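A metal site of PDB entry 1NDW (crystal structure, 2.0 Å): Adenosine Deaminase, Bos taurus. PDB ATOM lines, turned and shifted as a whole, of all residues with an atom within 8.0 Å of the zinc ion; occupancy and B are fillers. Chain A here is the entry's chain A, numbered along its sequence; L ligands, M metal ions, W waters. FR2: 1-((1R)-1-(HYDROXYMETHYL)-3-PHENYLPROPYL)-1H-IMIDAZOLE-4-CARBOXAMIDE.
ND1 of His 16 is in hydrogen-bond range of O15 of the ligand (2.7 Å).
OD1 of Asp 295 lies within hydrogen-bond range of N4 of the ligand.
Water W1 bridges OD1 of Asp 294 (2.5 Å) and NE2 of His 237 (2.7 Å).
A ring nitrogen (ND1) of His 14 lies close to the guanidinium group (NH1) of Arg 100, 3.4 Å away.
The side-chain carboxylate (OD1) of Asp 180 sits close to a ring nitrogen (ND1) of His 213.
OE1 of Glu 259 is in hydrogen-bond range of ND1 of His 14, 2.8 Å away.
The side-chain carboxylate (OD1) of Asp 294 is in hydrogen-bond range of the side-chain hydroxyl (OG) of Ser 264 (2.8 Å).
The backbone NH of His 213 lies within hydrogen-bond range of the backbone carbonyl oxygen of Leu 181, at 2.8 Å.
Four residues have an atom within 4 Å of the zinc ion: His 14, His 16, His 213 and Asp 294.
NE2 of His 16 binds the zinc ion, at 1.9 Å.
The zinc ion is bound by water W1, at 1.9 Å.
NE2 of His 14 binds the zinc ion (2.0 Å).
The zinc ion is bound by a ring nitrogen (NE2) of His 213, 2.2 Å away.
The zinc ion is bound by OD2 of Asp 294.
The zinc ion has five donor atoms within binding distance.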
ATOM      1  N   HIS A  14      21.313   6.333  19.159  1.00  0.00           N
ATOM      2  CA  HIS A  14      21.353   7.647  18.471  1.00  0.00           C
ATOM      3  C   HIS A  14      19.938   8.262  18.110  1.00  0.00           C
ATOM      4  O   HIS A  14      19.485   8.138  17.006  1.00  0.00           O
ATOM      5  CB  HIS A  14      22.288   7.590  17.202  1.00  0.00           C
ATOM      6  CG  HIS A  14      22.743   8.965  16.673  1.00  0.00           C
ATOM      7  ND1 HIS A  14      23.986   9.365  16.571  1.00  0.00           N
ATOM      8  CD2 HIS A  14      22.021  10.089  16.254  1.00  0.00           C
ATOM      9  CE1 HIS A  14      23.999  10.672  16.110  1.00  0.00           C
ATOM     10  NE2 HIS A  14      22.811  11.169  15.890  1.00  0.00           N
ATOM     11  N   VAL A  15      19.419   9.047  19.013  1.00  0.00           N
ATOM     12  CA  VAL A  15      18.183   9.710  18.898  1.00  0.00           C
ATOM     13  C   VAL A  15      18.193  11.002  19.786  1.00  0.00           C
ATOM     14  O   VAL A  15      18.567  11.047  20.939  1.00  0.00           O
ATOM     15  CB  VAL A  15      16.952   8.780  19.357  1.00  0.00           C
ATOM     16  CG1 VAL A  15      17.173   8.122  20.739  1.00  0.00           C
ATOM     17  CG2 VAL A  15      15.675   9.678  19.054  1.00  0.00           C
ATOM     18  N   HIS A  16      17.735  12.130  19.119  1.00  0.00           N
ATOM     19  CA  HIS A  16      17.827  13.381  19.837  1.00  0.00           C
ATOM     20  C   HIS A  16      16.462  13.688  20.474  1.00  0.00           C
ATOM     21  O   HIS A  16      15.481  13.761  19.747  1.00  0.00           O
ATOM     22  CB  HIS A  16      18.088  14.638  18.778  1.00  0.00           C
ATOM     23  CG  HIS A  16      19.397  14.506  17.978  1.00  0.00           C
ATOM     24  ND1 HIS A  16      20.398  15.346  18.276  1.00  0.00           N
ATOM     25  CD2 HIS A  16      19.896  13.617  17.056  1.00  0.00           C
ATOM     26  CE1 HIS A  16      21.500  14.989  17.533  1.00  0.00           C
ATOM     27  NE2 HIS A  16      21.271  13.921  16.769  1.00  0.00           N
ATOM     28  N   ARG A 100      19.808  11.887  23.532  1.00  0.00           N
ATOM     29  CA  ARG A 100      20.734  12.993  23.601  1.00  0.00           C
ATOM     30  C   ARG A 100      20.042  14.292  23.259  1.00  0.00           C
ATOM     31  O   ARG A 100      19.113  14.337  22.480  1.00  0.00           O
ATOM     32  CB  ARG A 100      21.920  12.835  22.591  1.00  0.00           C
ATOM     33  CG  ARG A 100      21.410  12.826  21.059  1.00  0.00           C
ATOM     34  CD  ARG A 100      22.808  12.617  20.275  1.00  0.00           C
ATOM     35  NE  ARG A 100      23.157  11.162  20.466  1.00  0.00           N
ATOM     36  CZ  ARG A 100      24.279  10.565  19.953  1.00  0.00           C
ATOM     37  NH1 ARG A 100      25.060  11.311  19.150  1.00  0.00           N
ATOM     38  NH2 ARG A 100      24.560   9.223  20.136  1.00  0.00           N
ATOM     39  N   CYS A 152      24.876  17.179  24.601  1.00  0.00           N
ATOM     40  CA  CYS A 152      25.631  17.574  23.437  1.00  0.00           C
ATOM     41  C   CYS A 152      26.241  18.955  23.672  1.00  0.00           C
ATOM     42  O   CYS A 152      25.542  19.924  23.910  1.00  0.00           O
ATOM     43  CB  CYS A 152      24.579  17.753  22.262  1.00  0.00           C
ATOM     44  SG  CYS A 152      23.535  16.251  21.878  1.00  0.00           S
ATOM     45  N   ASP A 180      28.420  14.461  23.754  1.00  0.00           N
ATOM     46  CA  ASP A 180      28.447  14.336  22.328  1.00  0.00           C
ATOM     47  C   ASP A 180      28.800  15.736  21.784  1.00  0.00           C
ATOM     48  O   ASP A 180      28.801  16.777  22.477  1.00  0.00           O
ATOM     49  CB  ASP A 180      26.979  13.945  21.883  1.00  0.00           C
ATOM     50  CG  ASP A 180      26.774  13.812  20.279  1.00  0.00           C
ATOM     51  OD1 ASP A 180      25.672  14.109  19.840  1.00  0.00           O
ATOM     52  OD2 ASP A 180      27.697  13.430  19.533  1.00  0.00           O
ATOM     53  N   LEU A 181      29.049  15.674  20.541  1.00  0.00           N
ATOM     54  CA  LEU A 181      29.258  16.952  19.776  1.00  0.00           C
ATOM     55  C   LEU A 181      28.387  16.955  18.526  1.00  0.00           C
ATOM     56  O   LEU A 181      28.533  16.048  17.663  1.00  0.00           O
ATOM     57  CB  LEU A 181      30.817  17.050  19.426  1.00  0.00           C
ATOM     58  CG  LEU A 181      31.182  18.302  18.457  1.00  0.00           C
ATOM     59  CD1 LEU A 181      31.015  19.676  19.212  1.00  0.00           C
ATOM     60  CD2 LEU A 181      32.691  18.299  18.228  1.00  0.00           C
ATOM     61  N   ALA A 182      27.470  17.931  18.574  1.00  0.00           N
ATOM     62  CA  ALA A 182      26.383  17.923  17.580  1.00  0.00           C
ATOM     63  C   ALA A 182      26.431  19.318  16.876  1.00  0.00           C
ATOM     64  O   ALA A 182      27.188  20.170  17.227  1.00  0.00           O
ATOM     65  CB  ALA A 182      24.905  17.805  18.332  1.00  0.00           C
ATOM     66  N   GLY A 183      25.658  19.458  15.779  1.00  0.00           N
ATOM     67  CA  GLY A 183      25.456  20.632  14.852  1.00  0.00           C
ATOM     68  C   GLY A 183      26.197  20.565  13.541  1.00  0.00           C
ATOM     69  O   GLY A 183      26.254  19.575  12.847  1.00  0.00           O
ATOM     70  N   HIS A 213      29.314  13.521  16.623  1.00  0.00           N
ATOM     71  CA  HIS A 213      28.884  13.330  15.210  1.00  0.00           C
ATOM     72  C   HIS A 213      29.963  13.620  14.117  1.00  0.00           C
ATOM     73  O   HIS A 213      30.521  14.702  14.051  1.00  0.00           O
ATOM     74  CB  HIS A 213      27.675  14.362  14.944  1.00  0.00           C
ATOM     75  CG  HIS A 213      26.387  13.996  15.682  1.00  0.00           C
ATOM     76  ND1 HIS A 213      26.201  14.039  17.010  1.00  0.00           N
ATOM     77  CD2 HIS A 213      25.116  13.886  15.051  1.00  0.00           C
ATOM     78  CE1 HIS A 213      24.920  14.010  17.175  1.00  0.00           C
ATOM     79  NE2 HIS A 213      24.192  13.962  16.016  1.00  0.00           N
ATOM     80  N   GLU A 216      29.109  12.427   8.740  1.00  0.00           N
ATOM     81  CA  GLU A 216      27.712  12.271   8.193  1.00  0.00           C
ATOM     82  C   GLU A 216      27.576  13.064   6.872  1.00  0.00           C
ATOM     83  O   GLU A 216      27.305  12.602   5.791  1.00  0.00           O
ATOM     84  CB  GLU A 216      26.667  12.855   9.153  1.00  0.00           C
ATOM     85  CG  GLU A 216      25.165  12.994   8.599  1.00  0.00           C
ATOM     86  CD  GLU A 216      24.267  13.815   9.540  1.00  0.00           C
ATOM     87  OE1 GLU A 216      24.769  14.383  10.480  1.00  0.00           O
ATOM     88  OE2 GLU A 216      23.032  13.881   9.432  1.00  0.00           O
ATOM     89  N   GLY A 236      28.812   9.242  15.514  1.00  0.00           N
ATOM     90  CA  GLY A 236      27.460   9.460  15.060  1.00  0.00           C
ATOM     91  C   GLY A 236      27.589   9.444  13.470  1.00  0.00           C
ATOM     92  O   GLY A 236      28.272  10.300  12.961  1.00  0.00           O
ATOM     93  N   HIS A 237      26.918   8.424  12.821  1.00  0.00           N
ATOM     94  CA  HIS A 237      27.023   8.164  11.370  1.00  0.00           C
ATOM     95  C   HIS A 237      28.359   7.639  10.890  1.00  0.00           C
ATOM     96  O   HIS A 237      28.648   6.456  10.714  1.00  0.00           O
ATOM     97  CB  HIS A 237      26.622   9.443  10.552  1.00  0.00           C
ATOM     98  CG  HIS A 237      25.324  10.076  10.996  1.00  0.00           C
ATOM     99  ND1 HIS A 237      24.064   9.747  10.591  1.00  0.00           N
ATOM    100  CD2 HIS A 237      25.124  11.110  11.840  1.00  0.00           C
ATOM    101  CE1 HIS A 237      23.147  10.477  11.161  1.00  0.00           C
ATOM    102  NE2 HIS A 237      23.749  11.366  11.943  1.00  0.00           N
ATOM    103  N   GLU A 259      27.179   4.679  14.810  1.00  0.00           N
ATOM    104  CA  GLU A 259      25.722   4.896  15.044  1.00  0.00           C
ATOM    105  C   GLU A 259      25.004   5.264  13.783  1.00  0.00           C
ATOM    106  O   GLU A 259      25.064   6.413  13.393  1.00  0.00           O
ATOM    107  CB  GLU A 259      25.556   6.098  15.971  1.00  0.00           C
ATOM    108  CG  GLU A 259      26.366   5.782  17.325  1.00  0.00           C
ATOM    109  CD  GLU A 259      26.476   6.973  18.279  1.00  0.00           C
ATOM    110  OE1 GLU A 259      26.023   8.033  17.865  1.00  0.00           O
ATOM    111  OE2 GLU A 259      27.077   6.927  19.404  1.00  0.00           O
ATOM    112  N   CYS A 261      22.098   5.816  10.852  1.00  0.00           N
ATOM    113  CA  CYS A 261      20.769   6.320  10.905  1.00  0.00           C
ATOM    114  C   CYS A 261      20.173   6.432   9.435  1.00  0.00           C
ATOM    115  O   CYS A 261      20.187   7.527   8.917  1.00  0.00           O
ATOM    116  CB  CYS A 261      20.775   7.752  11.438  1.00  0.00           C
ATOM    117  SG  CYS A 261      21.392   8.031  13.103  1.00  0.00           S
ATOM    118  N   SER A 264      16.994   8.947   8.183  1.00  0.00           N
ATOM    119  CA  SER A 264      17.709  10.211   8.313  1.00  0.00           C
ATOM    120  C   SER A 264      18.738  10.429   7.172  1.00  0.00           C
ATOM    121  O   SER A 264      18.687  11.522   6.613  1.00  0.00           O
ATOM    122  CB  SER A 264      18.541  10.210   9.626  1.00  0.00           C
ATOM    123  OG  SER A 264      19.295  11.371   9.794  1.00  0.00           O
ATOM    124  N   THR A 293      17.209   6.075  14.804  1.00  0.00           N
ATOM    125  CA  THR A 293      16.172   6.981  14.208  1.00  0.00           C
ATOM    126  C   THR A 293      16.554   8.472  13.995  1.00  0.00           C
ATOM    127  O   THR A 293      15.951   9.110  13.142  1.00  0.00           O
ATOM    128  CB  THR A 293      14.964   6.867  15.158  1.00  0.00           C
ATOM    129  OG1 THR A 293      13.941   5.875  14.804  1.00  0.00           O
ATOM    130  CG2 THR A 293      14.791   7.804  16.256  1.00  0.00           C
ATOM    131  N   ASP A 294      17.580   8.970  14.806  1.00  0.00           N
ATOM    132  CA  ASP A 294      18.030  10.395  14.836  1.00  0.00           C
ATOM    133  C   ASP A 294      16.974  11.399  15.363  1.00  0.00           C
ATOM    134  O   ASP A 294      16.983  11.890  16.495  1.00  0.00           O
ATOM    135  CB  ASP A 294      18.642  10.594  13.384  1.00  0.00           C
ATOM    136  CG  ASP A 294      19.705  11.692  13.415  1.00  0.00           C
ATOM    137  OD1 ASP A 294      20.228  12.079  12.322  1.00  0.00           O
ATOM    138  OD2 ASP A 294      19.997  12.097  14.533  1.00  0.00           O
ATOM    139  N   ASP A 295      15.925  11.690  14.447  1.00  0.00           N
ATOM    140  CA  ASP A 295      14.929  12.732  14.709  1.00  0.00           C
ATOM    141  C   ASP A 295      13.532  12.209  14.131  1.00  0.00           C
ATOM    142  O   ASP A 295      13.066  12.586  13.037  1.00  0.00           O
ATOM    143  CB  ASP A 295      15.258  14.096  14.024  1.00  0.00           C
ATOM    144  CG  ASP A 295      16.562  14.567  14.508  1.00  0.00           C
ATOM    145  OD1 ASP A 295      16.519  15.435  15.371  1.00  0.00           O
ATOM    146  OD2 ASP A 295      17.575  13.986  14.107  1.00  0.00           O
ATOM    147  N   PHE A 299      11.650  13.309  10.736  1.00  0.00           N
ATOM    148  CA  PHE A 299      11.588  12.375   9.673  1.00  0.00           C
ATOM    149  C   PHE A 299      10.254  11.555   9.481  1.00  0.00           C
ATOM    150  O   PHE A 299      10.370  10.629   8.686  1.00  0.00           O
ATOM    151  CB  PHE A 299      12.841  11.433   9.776  1.00  0.00           C
ATOM    152  CG  PHE A 299      14.133  12.280   9.929  1.00  0.00           C
ATOM    153  CD1 PHE A 299      14.311  13.494   9.164  1.00  0.00           C
ATOM    154  CD2 PHE A 299      15.157  11.839  10.826  1.00  0.00           C
ATOM    155  CE1 PHE A 299      15.582  14.219   9.143  1.00  0.00           C
ATOM    156  CE2 PHE A 299      16.373  12.609  10.829  1.00  0.00           C
ATOM    157  CZ  PHE A 299      16.620  13.730   9.976  1.00  0.00           C
HETATM  158  C1  FR2 L   1      20.589  18.237  16.120  1.00  0.00           C
HETATM  159  N2  FR2 L   1      19.670  18.402  17.233  1.00  0.00           N
HETATM  160  C3  FR2 L   1      18.658  17.582  17.048  1.00  0.00           C
HETATM  161  N4  FR2 L   1      18.774  16.911  15.958  1.00  0.00           N
HETATM  162  C5  FR2 L   1      20.009  17.326  15.346  1.00  0.00           C
HETATM  163  C8  FR2 L   1      20.598  16.794  14.115  1.00  0.00           C
HETATM  164  O9  FR2 L   1      21.668  17.223  13.651  1.00  0.00           O
HETATM  165  N10 FR2 L   1      19.915  15.889  13.421  1.00  0.00           N
HETATM  166  C13 FR2 L   1      19.768  19.434  18.281  1.00  0.00           C
HETATM  167  C14 FR2 L   1      20.671  18.947  19.444  1.00  0.00           C
HETATM  168  O15 FR2 L   1      20.066  17.633  19.664  1.00  0.00           O
HETATM  169  C18 FR2 L   1      20.224  20.823  17.818  1.00  0.00           C
HETATM  170  C19 FR2 L   1      19.367  21.338  16.621  1.00  0.00           C
HETATM  171  C22 FR2 L   1      19.647  22.782  16.244  1.00  0.00           C
HETATM  172  C25 FR2 L   1      18.986  23.329  15.163  1.00  0.00           C
HETATM  173  C26 FR2 L   1      19.191  24.650  14.781  1.00  0.00           C
HETATM  174  C27 FR2 L   1      20.136  25.432  15.452  1.00  0.00           C
HETATM  175  C28 FR2 L   1      20.847  24.908  16.543  1.00  0.00           C
HETATM  176  C29 FR2 L   1      20.556  23.580  16.925  1.00  0.00           C
HETATM  177 ZN    ZN M   1      22.251  13.054  15.402  1.00  0.00          ZN
HETATM  178  O   HOH W   1      22.268  13.069  13.476  1.00  0.00           O
